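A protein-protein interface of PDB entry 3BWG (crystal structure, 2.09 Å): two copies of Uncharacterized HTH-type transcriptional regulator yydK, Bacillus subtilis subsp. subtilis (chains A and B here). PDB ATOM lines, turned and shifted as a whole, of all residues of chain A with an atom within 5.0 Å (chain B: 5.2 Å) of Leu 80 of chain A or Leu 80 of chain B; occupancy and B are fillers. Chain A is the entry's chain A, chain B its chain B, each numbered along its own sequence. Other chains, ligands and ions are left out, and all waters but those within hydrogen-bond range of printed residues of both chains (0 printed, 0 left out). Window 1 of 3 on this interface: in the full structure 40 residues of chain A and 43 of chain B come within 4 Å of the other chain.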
ATOM      1  N   ILE A  78     -25.334 -15.594 -30.976  1.00  0.00           N
ATOM      2  CA  ILE A  78     -25.137 -17.038 -31.076  1.00  0.00           C
ATOM      3  C   ILE A  78     -26.339 -17.633 -30.350  1.00  0.00           C
ATOM      4  O   ILE A  78     -26.646 -17.200 -29.262  1.00  0.00           O
ATOM      5  CB  ILE A  78     -23.821 -17.445 -30.359  1.00  0.00           C
ATOM      6  CG1 ILE A  78     -22.600 -16.986 -31.169  1.00  0.00           C
ATOM      7  CG2 ILE A  78     -23.733 -18.956 -30.104  1.00  0.00           C
ATOM      8  CD1 ILE A  78     -21.360 -16.843 -30.296  1.00  0.00           C
ATOM      9  N   SER A  79     -27.053 -18.585 -30.954  1.00  0.00           N
ATOM     10  CA  SER A  79     -28.110 -19.212 -30.196  1.00  0.00           C
ATOM     11  C   SER A  79     -27.561 -20.089 -29.024  1.00  0.00           C
ATOM     12  O   SER A  79     -26.696 -20.961 -29.165  1.00  0.00           O
ATOM     13  CB  SER A  79     -29.140 -19.898 -31.095  1.00  0.00           C
ATOM     14  OG  SER A  79     -28.583 -21.049 -31.625  1.00  0.00           O
ATOM     15  N   LEU A  80     -28.033 -19.774 -27.831  1.00  0.00           N
ATOM     16  CA  LEU A  80     -27.558 -20.453 -26.610  1.00  0.00           C
ATOM     17  C   LEU A  80     -27.780 -21.981 -26.701  1.00  0.00           C
ATOM     18  O   LEU A  80     -26.898 -22.784 -26.371  1.00  0.00           O
ATOM     19  CB  LEU A  80     -28.267 -19.850 -25.395  1.00  0.00           C
ATOM     20  CG  LEU A  80     -27.764 -20.197 -23.977  1.00  0.00           C
ATOM     21  CD1 LEU A  80     -26.360 -19.636 -23.720  1.00  0.00           C
ATOM     22  CD2 LEU A  80     -28.754 -19.739 -22.914  1.00  0.00           C
ATOM     23  N   LEU A  81     -28.969 -22.353 -27.158  1.00  0.00           N
ATOM     24  CA  LEU A  81     -29.401 -23.734 -27.172  1.00  0.00           C
ATOM     25  C   LEU A  81     -29.127 -24.293 -28.554  1.00  0.00           C
ATOM     26  O   LEU A  81     -29.660 -23.798 -29.530  1.00  0.00           O
ATOM     27  CB  LEU A  81     -30.890 -23.809 -26.833  1.00  0.00           C
ATOM     28  CG  LEU A  81     -31.221 -23.098 -25.521  1.00  0.00           C
ATOM     29  CD1 LEU A  81     -32.681 -22.928 -25.346  1.00  0.00           C
ATOM     30  CD2 LEU A  81     -30.590 -23.797 -24.321  1.00  0.00           C
ATOM     31  N   SER A  82     -28.279 -25.315 -28.606  1.00  0.00           N
ATOM     32  CA  SER A  82     -27.791 -25.891 -29.847  1.00  0.00           C
ATOM     33  C   SER A  82     -28.919 -26.023 -30.859  1.00  0.00           C
ATOM     34  O   SER A  82     -28.860 -25.428 -31.944  1.00  0.00           O
ATOM     35  CB  SER A  82     -27.088 -27.236 -29.576  1.00  0.00           C
ATOM     36  OG  SER A  82     -26.025 -27.090 -28.633  1.00  0.00           O
ATOM     37  N   LEU A 178     -28.124 -26.585 -19.177  1.00  0.00           N
ATOM     38  CA  LEU A 178     -27.014 -25.625 -19.168  1.00  0.00           C
ATOM     39  C   LEU A 178     -27.080 -24.820 -17.864  1.00  0.00           C
ATOM     40  O   LEU A 178     -28.146 -24.329 -17.470  1.00  0.00           O
ATOM     41  CB  LEU A 178     -27.129 -24.663 -20.326  1.00  0.00           C
ATOM     42  CG  LEU A 178     -26.716 -25.034 -21.760  1.00  0.00           C
ATOM     43  CD1 LEU A 178     -27.364 -26.284 -22.314  1.00  0.00           C
ATOM     44  CD2 LEU A 178     -26.982 -23.832 -22.689  1.00  0.00           C
ATOM     45  N   LEU A 180     -25.173 -21.696 -16.046  1.00  0.00           N
ATOM     46  CA  LEU A 180     -24.502 -20.538 -16.548  1.00  0.00           C
ATOM     47  C   LEU A 180     -24.047 -19.733 -15.335  1.00  0.00           C
ATOM     48  O   LEU A 180     -24.856 -19.474 -14.422  1.00  0.00           O
ATOM     49  CB  LEU A 180     -25.467 -19.691 -17.346  1.00  0.00           C
ATOM     50  CG  LEU A 180     -25.919 -20.020 -18.787  1.00  0.00           C
ATOM     51  CD1 LEU A 180     -26.964 -21.105 -18.843  1.00  0.00           C
ATOM     52  CD2 LEU A 180     -26.508 -18.747 -19.373  1.00  0.00           C
ATOM     53  N   ILE A 204     -20.091 -21.818 -18.702  1.00  0.00           N
ATOM     54  CA  ILE A 204     -21.266 -22.699 -18.822  1.00  0.00           C
ATOM     55  C   ILE A 204     -20.848 -24.153 -18.622  1.00  0.00           C
ATOM     56  O   ILE A 204     -19.875 -24.616 -19.276  1.00  0.00           O
ATOM     57  CB  ILE A 204     -21.973 -22.528 -20.214  1.00  0.00           C
ATOM     58  CG1 ILE A 204     -22.443 -21.085 -20.382  1.00  0.00           C
ATOM     59  CG2 ILE A 204     -23.246 -23.412 -20.300  1.00  0.00           C
ATOM     60  CD1 ILE A 204     -23.307 -20.843 -21.699  1.00  0.00           C
ATOM     61  N   PHE A 230     -25.509 -13.942 -26.854  1.00  0.00           N
ATOM     62  CA  PHE A 230     -26.365 -15.110 -27.024  1.00  0.00           C
ATOM     63  C   PHE A 230     -27.814 -14.735 -27.083  1.00  0.00           C
ATOM     64  O   PHE A 230     -28.193 -13.705 -26.575  1.00  0.00           O
ATOM     65  CB  PHE A 230     -26.118 -16.109 -25.876  1.00  0.00           C
ATOM     66  CG  PHE A 230     -24.682 -16.526 -25.777  1.00  0.00           C
ATOM     67  CD1 PHE A 230     -24.209 -17.609 -26.532  1.00  0.00           C
ATOM     68  CD2 PHE A 230     -23.782 -15.774 -24.997  1.00  0.00           C
ATOM     69  CE1 PHE A 230     -22.831 -17.958 -26.476  1.00  0.00           C
ATOM     70  CE2 PHE A 230     -22.414 -16.102 -24.922  1.00  0.00           C
ATOM     71  CZ  PHE A 230     -21.933 -17.196 -25.652  1.00  0.00           C
ATOM     72  N   VAL A 231     -28.610 -15.541 -27.777  1.00  0.00           N
ATOM     73  CA  VAL A 231     -30.030 -15.385 -27.770  1.00  0.00           C
ATOM     74  C   VAL A 231     -30.622 -16.703 -27.315  1.00  0.00           C
ATOM     75  O   VAL A 231     -30.145 -17.774 -27.652  1.00  0.00           O
ATOM     76  CB  VAL A 231     -30.640 -14.882 -29.127  1.00  0.00           C
ATOM     77  CG1 VAL A 231     -30.068 -15.653 -30.394  1.00  0.00           C
ATOM     78  CG2 VAL A 231     -32.181 -14.916 -29.094  1.00  0.00           C
ATOM     79  N   VAL A 232     -31.648 -16.605 -26.496  1.00  0.00           N
ATOM     80  CA  VAL A 232     -32.448 -17.774 -26.122  1.00  0.00           C
ATOM     81  C   VAL A 232     -33.903 -17.357 -26.179  1.00  0.00           C
ATOM     82  O   VAL A 232     -34.245 -16.184 -25.956  1.00  0.00           O
ATOM     83  CB  VAL A 232     -31.975 -18.419 -24.766  1.00  0.00           C
ATOM     84  CG1 VAL A 232     -31.943 -17.423 -23.673  1.00  0.00           C
ATOM     85  CG2 VAL A 232     -32.848 -19.669 -24.379  1.00  0.00           C
ATOM     86  N   ILE B  78     -31.201 -20.006 -10.711  1.00  0.00           N
ATOM     87  CA  ILE B  78     -32.395 -19.270 -11.147  1.00  0.00           C
ATOM     88  C   ILE B  78     -32.716 -19.733 -12.569  1.00  0.00           C
ATOM     89  O   ILE B  78     -31.837 -19.828 -13.453  1.00  0.00           O
ATOM     90  CB  ILE B  78     -32.201 -17.724 -11.166  1.00  0.00           C
ATOM     91  CG1 ILE B  78     -31.803 -17.181  -9.775  1.00  0.00           C
ATOM     92  CG2 ILE B  78     -33.463 -17.001 -11.748  1.00  0.00           C
ATOM     93  CD1 ILE B  78     -30.811 -16.020  -9.891  1.00  0.00           C
ATOM     94  N   SER B  79     -33.979 -20.059 -12.760  1.00  0.00           N
ATOM     95  CA  SER B  79     -34.481 -20.424 -14.052  1.00  0.00           C
ATOM     96  C   SER B  79     -34.372 -19.228 -15.018  1.00  0.00           C
ATOM     97  O   SER B  79     -34.995 -18.185 -14.848  1.00  0.00           O
ATOM     98  CB  SER B  79     -35.914 -20.928 -13.911  1.00  0.00           C
ATOM     99  OG  SER B  79     -36.421 -21.110 -15.220  1.00  0.00           O
ATOM    100  N   LEU B  80     -33.511 -19.356 -16.003  1.00  0.00           N
ATOM    101  CA  LEU B  80     -33.290 -18.243 -16.912  1.00  0.00           C
ATOM    102  C   LEU B  80     -34.585 -17.876 -17.651  1.00  0.00           C
ATOM    103  O   LEU B  80     -34.899 -16.690 -17.810  1.00  0.00           O
ATOM    104  CB  LEU B  80     -32.172 -18.606 -17.882  1.00  0.00           C
ATOM    105  CG  LEU B  80     -31.724 -17.576 -18.918  1.00  0.00           C
ATOM    106  CD1 LEU B  80     -31.008 -16.383 -18.319  1.00  0.00           C
ATOM    107  CD2 LEU B  80     -30.862 -18.305 -19.904  1.00  0.00           C
ATOM    108  N   LEU B  81     -35.351 -18.887 -18.072  1.00  0.00           N
ATOM    109  CA  LEU B  81     -36.626 -18.686 -18.748  1.00  0.00           C
ATOM    110  C   LEU B  81     -37.780 -18.713 -17.735  1.00  0.00           C
ATOM    111  O   LEU B  81     -37.914 -19.666 -16.977  1.00  0.00           O
ATOM    112  CB  LEU B  81     -36.832 -19.749 -19.875  1.00  0.00           C
ATOM    113  CG  LEU B  81     -35.700 -19.840 -20.946  1.00  0.00           C
ATOM    114  CD1 LEU B  81     -35.985 -20.877 -22.036  1.00  0.00           C
ATOM    115  CD2 LEU B  81     -35.404 -18.479 -21.615  1.00  0.00           C
ATOM    116  N   SER B  82     -38.606 -17.673 -17.736  1.00  0.00           N
ATOM    117  CA  SER B  82     -39.657 -17.503 -16.727  1.00  0.00           C
ATOM    118  C   SER B  82     -40.813 -18.451 -16.993  1.00  0.00           C
ATOM    119  O   SER B  82     -41.260 -18.572 -18.136  1.00  0.00           O
ATOM    120  CB  SER B  82     -40.219 -16.066 -16.755  1.00  0.00           C
ATOM    121  OG  SER B  82     -39.190 -15.112 -16.997  1.00  0.00           O
ATOM    122  N   LEU B 178     -34.614 -13.451 -25.121  1.00  0.00           N
ATOM    123  CA  LEU B 178     -33.549 -12.927 -24.233  1.00  0.00           C
ATOM    124  C   LEU B 178     -32.233 -12.843 -24.972  1.00  0.00           C
ATOM    125  O   LEU B 178     -31.877 -13.799 -25.687  1.00  0.00           O
ATOM    126  CB  LEU B 178     -33.360 -13.793 -22.973  1.00  0.00           C
ATOM    127  CG  LEU B 178     -34.331 -13.714 -21.789  1.00  0.00           C
ATOM    128  CD1 LEU B 178     -35.804 -14.003 -22.257  1.00  0.00           C
ATOM    129  CD2 LEU B 178     -33.945 -14.630 -20.621  1.00  0.00           C
ATOM    130  N   LEU B 180     -28.252 -12.013 -24.200  1.00  0.00           N
ATOM    131  CA  LEU B 180     -27.284 -12.121 -23.089  1.00  0.00           C
ATOM    132  C   LEU B 180     -25.921 -11.600 -23.485  1.00  0.00           C
ATOM    133  O   LEU B 180     -25.404 -11.948 -24.543  1.00  0.00           O
ATOM    134  CB  LEU B 180     -27.155 -13.582 -22.631  1.00  0.00           C
ATOM    135  CG  LEU B 180     -28.229 -14.221 -21.741  1.00  0.00           C
ATOM    136  CD1 LEU B 180     -29.536 -14.523 -22.462  1.00  0.00           C
ATOM    137  CD2 LEU B 180     -27.691 -15.500 -21.181  1.00  0.00           C
ATOM    138  N   ILE B 204     -28.669  -8.804 -19.403  1.00  0.00           N
ATOM    139  CA  ILE B 204     -29.705  -9.417 -20.257  1.00  0.00           C
ATOM    140  C   ILE B 204     -30.731  -8.390 -20.644  1.00  0.00           C
ATOM    141  O   ILE B 204     -31.224  -7.655 -19.762  1.00  0.00           O
ATOM    142  CB  ILE B 204     -30.442 -10.584 -19.495  1.00  0.00           C
ATOM    143  CG1 ILE B 204     -29.417 -11.570 -18.913  1.00  0.00           C
ATOM    144  CG2 ILE B 204     -31.580 -11.281 -20.398  1.00  0.00           C
ATOM    145  CD1 ILE B 204     -30.019 -12.749 -18.250  1.00  0.00           C
ATOM    146  N   PHE B 230     -27.585 -19.394 -13.360  1.00  0.00           N
ATOM    147  CA  PHE B 230     -28.830 -19.702 -14.098  1.00  0.00           C
ATOM    148  C   PHE B 230     -28.863 -21.085 -14.713  1.00  0.00           C
ATOM    149  O   PHE B 230     -27.841 -21.613 -15.093  1.00  0.00           O
ATOM    150  CB  PHE B 230     -29.111 -18.644 -15.189  1.00  0.00           C
ATOM    151  CG  PHE B 230     -29.131 -17.246 -14.642  1.00  0.00           C
ATOM    152  CD1 PHE B 230     -30.324 -16.679 -14.183  1.00  0.00           C
ATOM    153  CD2 PHE B 230     -27.958 -16.510 -14.559  1.00  0.00           C
ATOM    154  CE1 PHE B 230     -30.349 -15.424 -13.595  1.00  0.00           C
ATOM    155  CE2 PHE B 230     -27.972 -15.220 -13.993  1.00  0.00           C
ATOM    156  CZ  PHE B 230     -29.204 -14.698 -13.494  1.00  0.00           C
ATOM    157  N   VAL B 231     -30.045 -21.670 -14.755  1.00  0.00           N
ATOM    158  CA  VAL B 231     -30.243 -22.894 -15.458  1.00  0.00           C
ATOM    159  C   VAL B 231     -31.287 -22.719 -16.581  1.00  0.00           C
ATOM    160  O   VAL B 231     -32.212 -21.881 -16.516  1.00  0.00           O
ATOM    161  CB  VAL B 231     -30.578 -24.095 -14.500  1.00  0.00           C
ATOM    162  CG1 VAL B 231     -31.880 -23.853 -13.628  1.00  0.00           C
ATOM    163  CG2 VAL B 231     -30.682 -25.373 -15.293  1.00  0.00           C
ATOM    164  N   VAL B 232     -31.094 -23.518 -17.631  1.00  0.00           N
ATOM    165  CA  VAL B 232     -32.048 -23.652 -18.691  1.00  0.00           C
ATOM    166  C   VAL B 232     -32.065 -25.094 -19.171  1.00  0.00           C
ATOM    167  O   VAL B 232     -31.002 -25.758 -19.301  1.00  0.00           O
ATOM    168  CB  VAL B 232     -31.843 -22.590 -19.807  1.00  0.00           C
ATOM    169  CG1 VAL B 232     -30.441 -22.431 -20.115  1.00  0.00           C
ATOM    170  CG2 VAL B 232     -32.749 -22.866 -21.048  1.00  0.00           C
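The backbone NH (N) of Leu 178 of chain A is in hydrogen-bond range of the backbone carbonyl oxygen (O) of Val 232 of chain B. The backbone NH of Leu 180 of chain A sits at hydrogen-bond distance from the backbone carbonyl oxygen of Phe 230 of chain B (2.8 Å). O of Phe 230 of chain A is in hydrogen-bond range of N of Leu 180 of chain B (2.9 Å). The backbone carbonyl oxygen of Val 232 of chain A is in hydrogen-bond range of the backbone NH of Leu 178 of chain B (2.9 Å).
The backbone carbonyl oxygen (O) of Ile 78 of chain A lies within hydrogen-bond range of the backbone NH (N) of Val 231 of chain A (3.0 Å). The backbone carbonyl oxygen of Val 231 of chain A lies within hydrogen-bond range of the backbone NH of Leu 80 of chain A (2.9 Å). The backbone NH (N) of Val 231 of chain B sits at hydrogen-bond distance from the backbone carbonyl oxygen (O) of Ile 78 of chain B, 2.9 Å away. The side-chain hydroxyl (OG) of Ser 79 of chain B lies within hydrogen-bond range of the backbone carbonyl oxygen (O) of Leu 81 of chain B. The backbone carbonyl oxygen (O) of Val 231 of chain B sits at hydrogen-bond distance from the backbone NH (N) of Leu 80 of chain B (2.9 Å).
Among the printed residues, merely in contact across the chains: Val 231 of chain A with Leu 178 of chain B (3.2 Å), Leu 178 of chain A with Val 231 of chain B (3.2 Å), Leu 178 of chain A with Phe 230 of chain B (3.6 Å), Phe 230 of chain A with Leu 178 of chain B (3.8 Å), Leu 180 of chain A with Leu 180 of chain B (3.9 Å), Leu 180 of chain A with Val 232 of chain B (3.9 Å), Leu 80 of chain A with Leu 80 of chain B (3.9 Å), Val 232 of chain A with Leu 81 of chain B (3.9 Å) and Val 232 of chain A with Leu 180 of chain B (3.96 Å).
Printed residues of chain B within 4 Å of Leu 80 of chain A: Leu 80 (3.9 Å). Of the printed residues of chain B, Leu 178 of chain A touches Phe 230 (3.6 Å), Val 231 (3.2 Å) and Val 232 (3.0 Å). Of the printed residues of chain B, Val 232 of chain A touches Leu 81, Leu 178 and Leu 180. Printed residues of chain A within 4 Å of Leu 80 of chain B: Leu 80. Ile 204 of chain B touches none of the printed residues of chain A. Of the printed residues of chain A, Phe 230 of chain B touches Leu 178 and Leu 180. The nearest printed residue of chain A that does not touch Leu 80 of chain B is Val 232 of chain A (4.02 Å).
Of the 11 printed residues of chain A, 6 touch a printed residue of chain B. Along chain A the printed residues that touch a printed residue of chain B span positions 80 to 232. Of the 11 printed residues of chain B, 7 touch a printed residue of chain A. Among the printed residues, no Asp or Glu carboxylate lies within 4 Å of a Lys or Arg side-chain nitrogen of the other chain.
Leu 178 of chain A touches Phe 230 of chain B, and with the chains exchanged Phe 230 of chain A touches Leu 178 of chain B. Leu 178 of chain A touches Val 232 of chain B, and with the chains exchanged Val 232 of chain A touches Leu 178 of chain B. Leu 180 of chain A touches Phe 230 of chain B, and with the chains exchanged Phe 230 of chain A touches Leu 180 of chain B. Val 232 of chain A touches Leu 81 of chain B, but with the chains exchanged Leu 81 of chain A does not touch Val 232 of chain B (4.03 Å). Positions printed for both chains: 78, 79, 80, 81, 82, 178, 180, 204, 230, 231 and 232. Of the 13 pairs that touch across the chains among the printed residues, 12 have their exchanged pair printed and touching as well.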
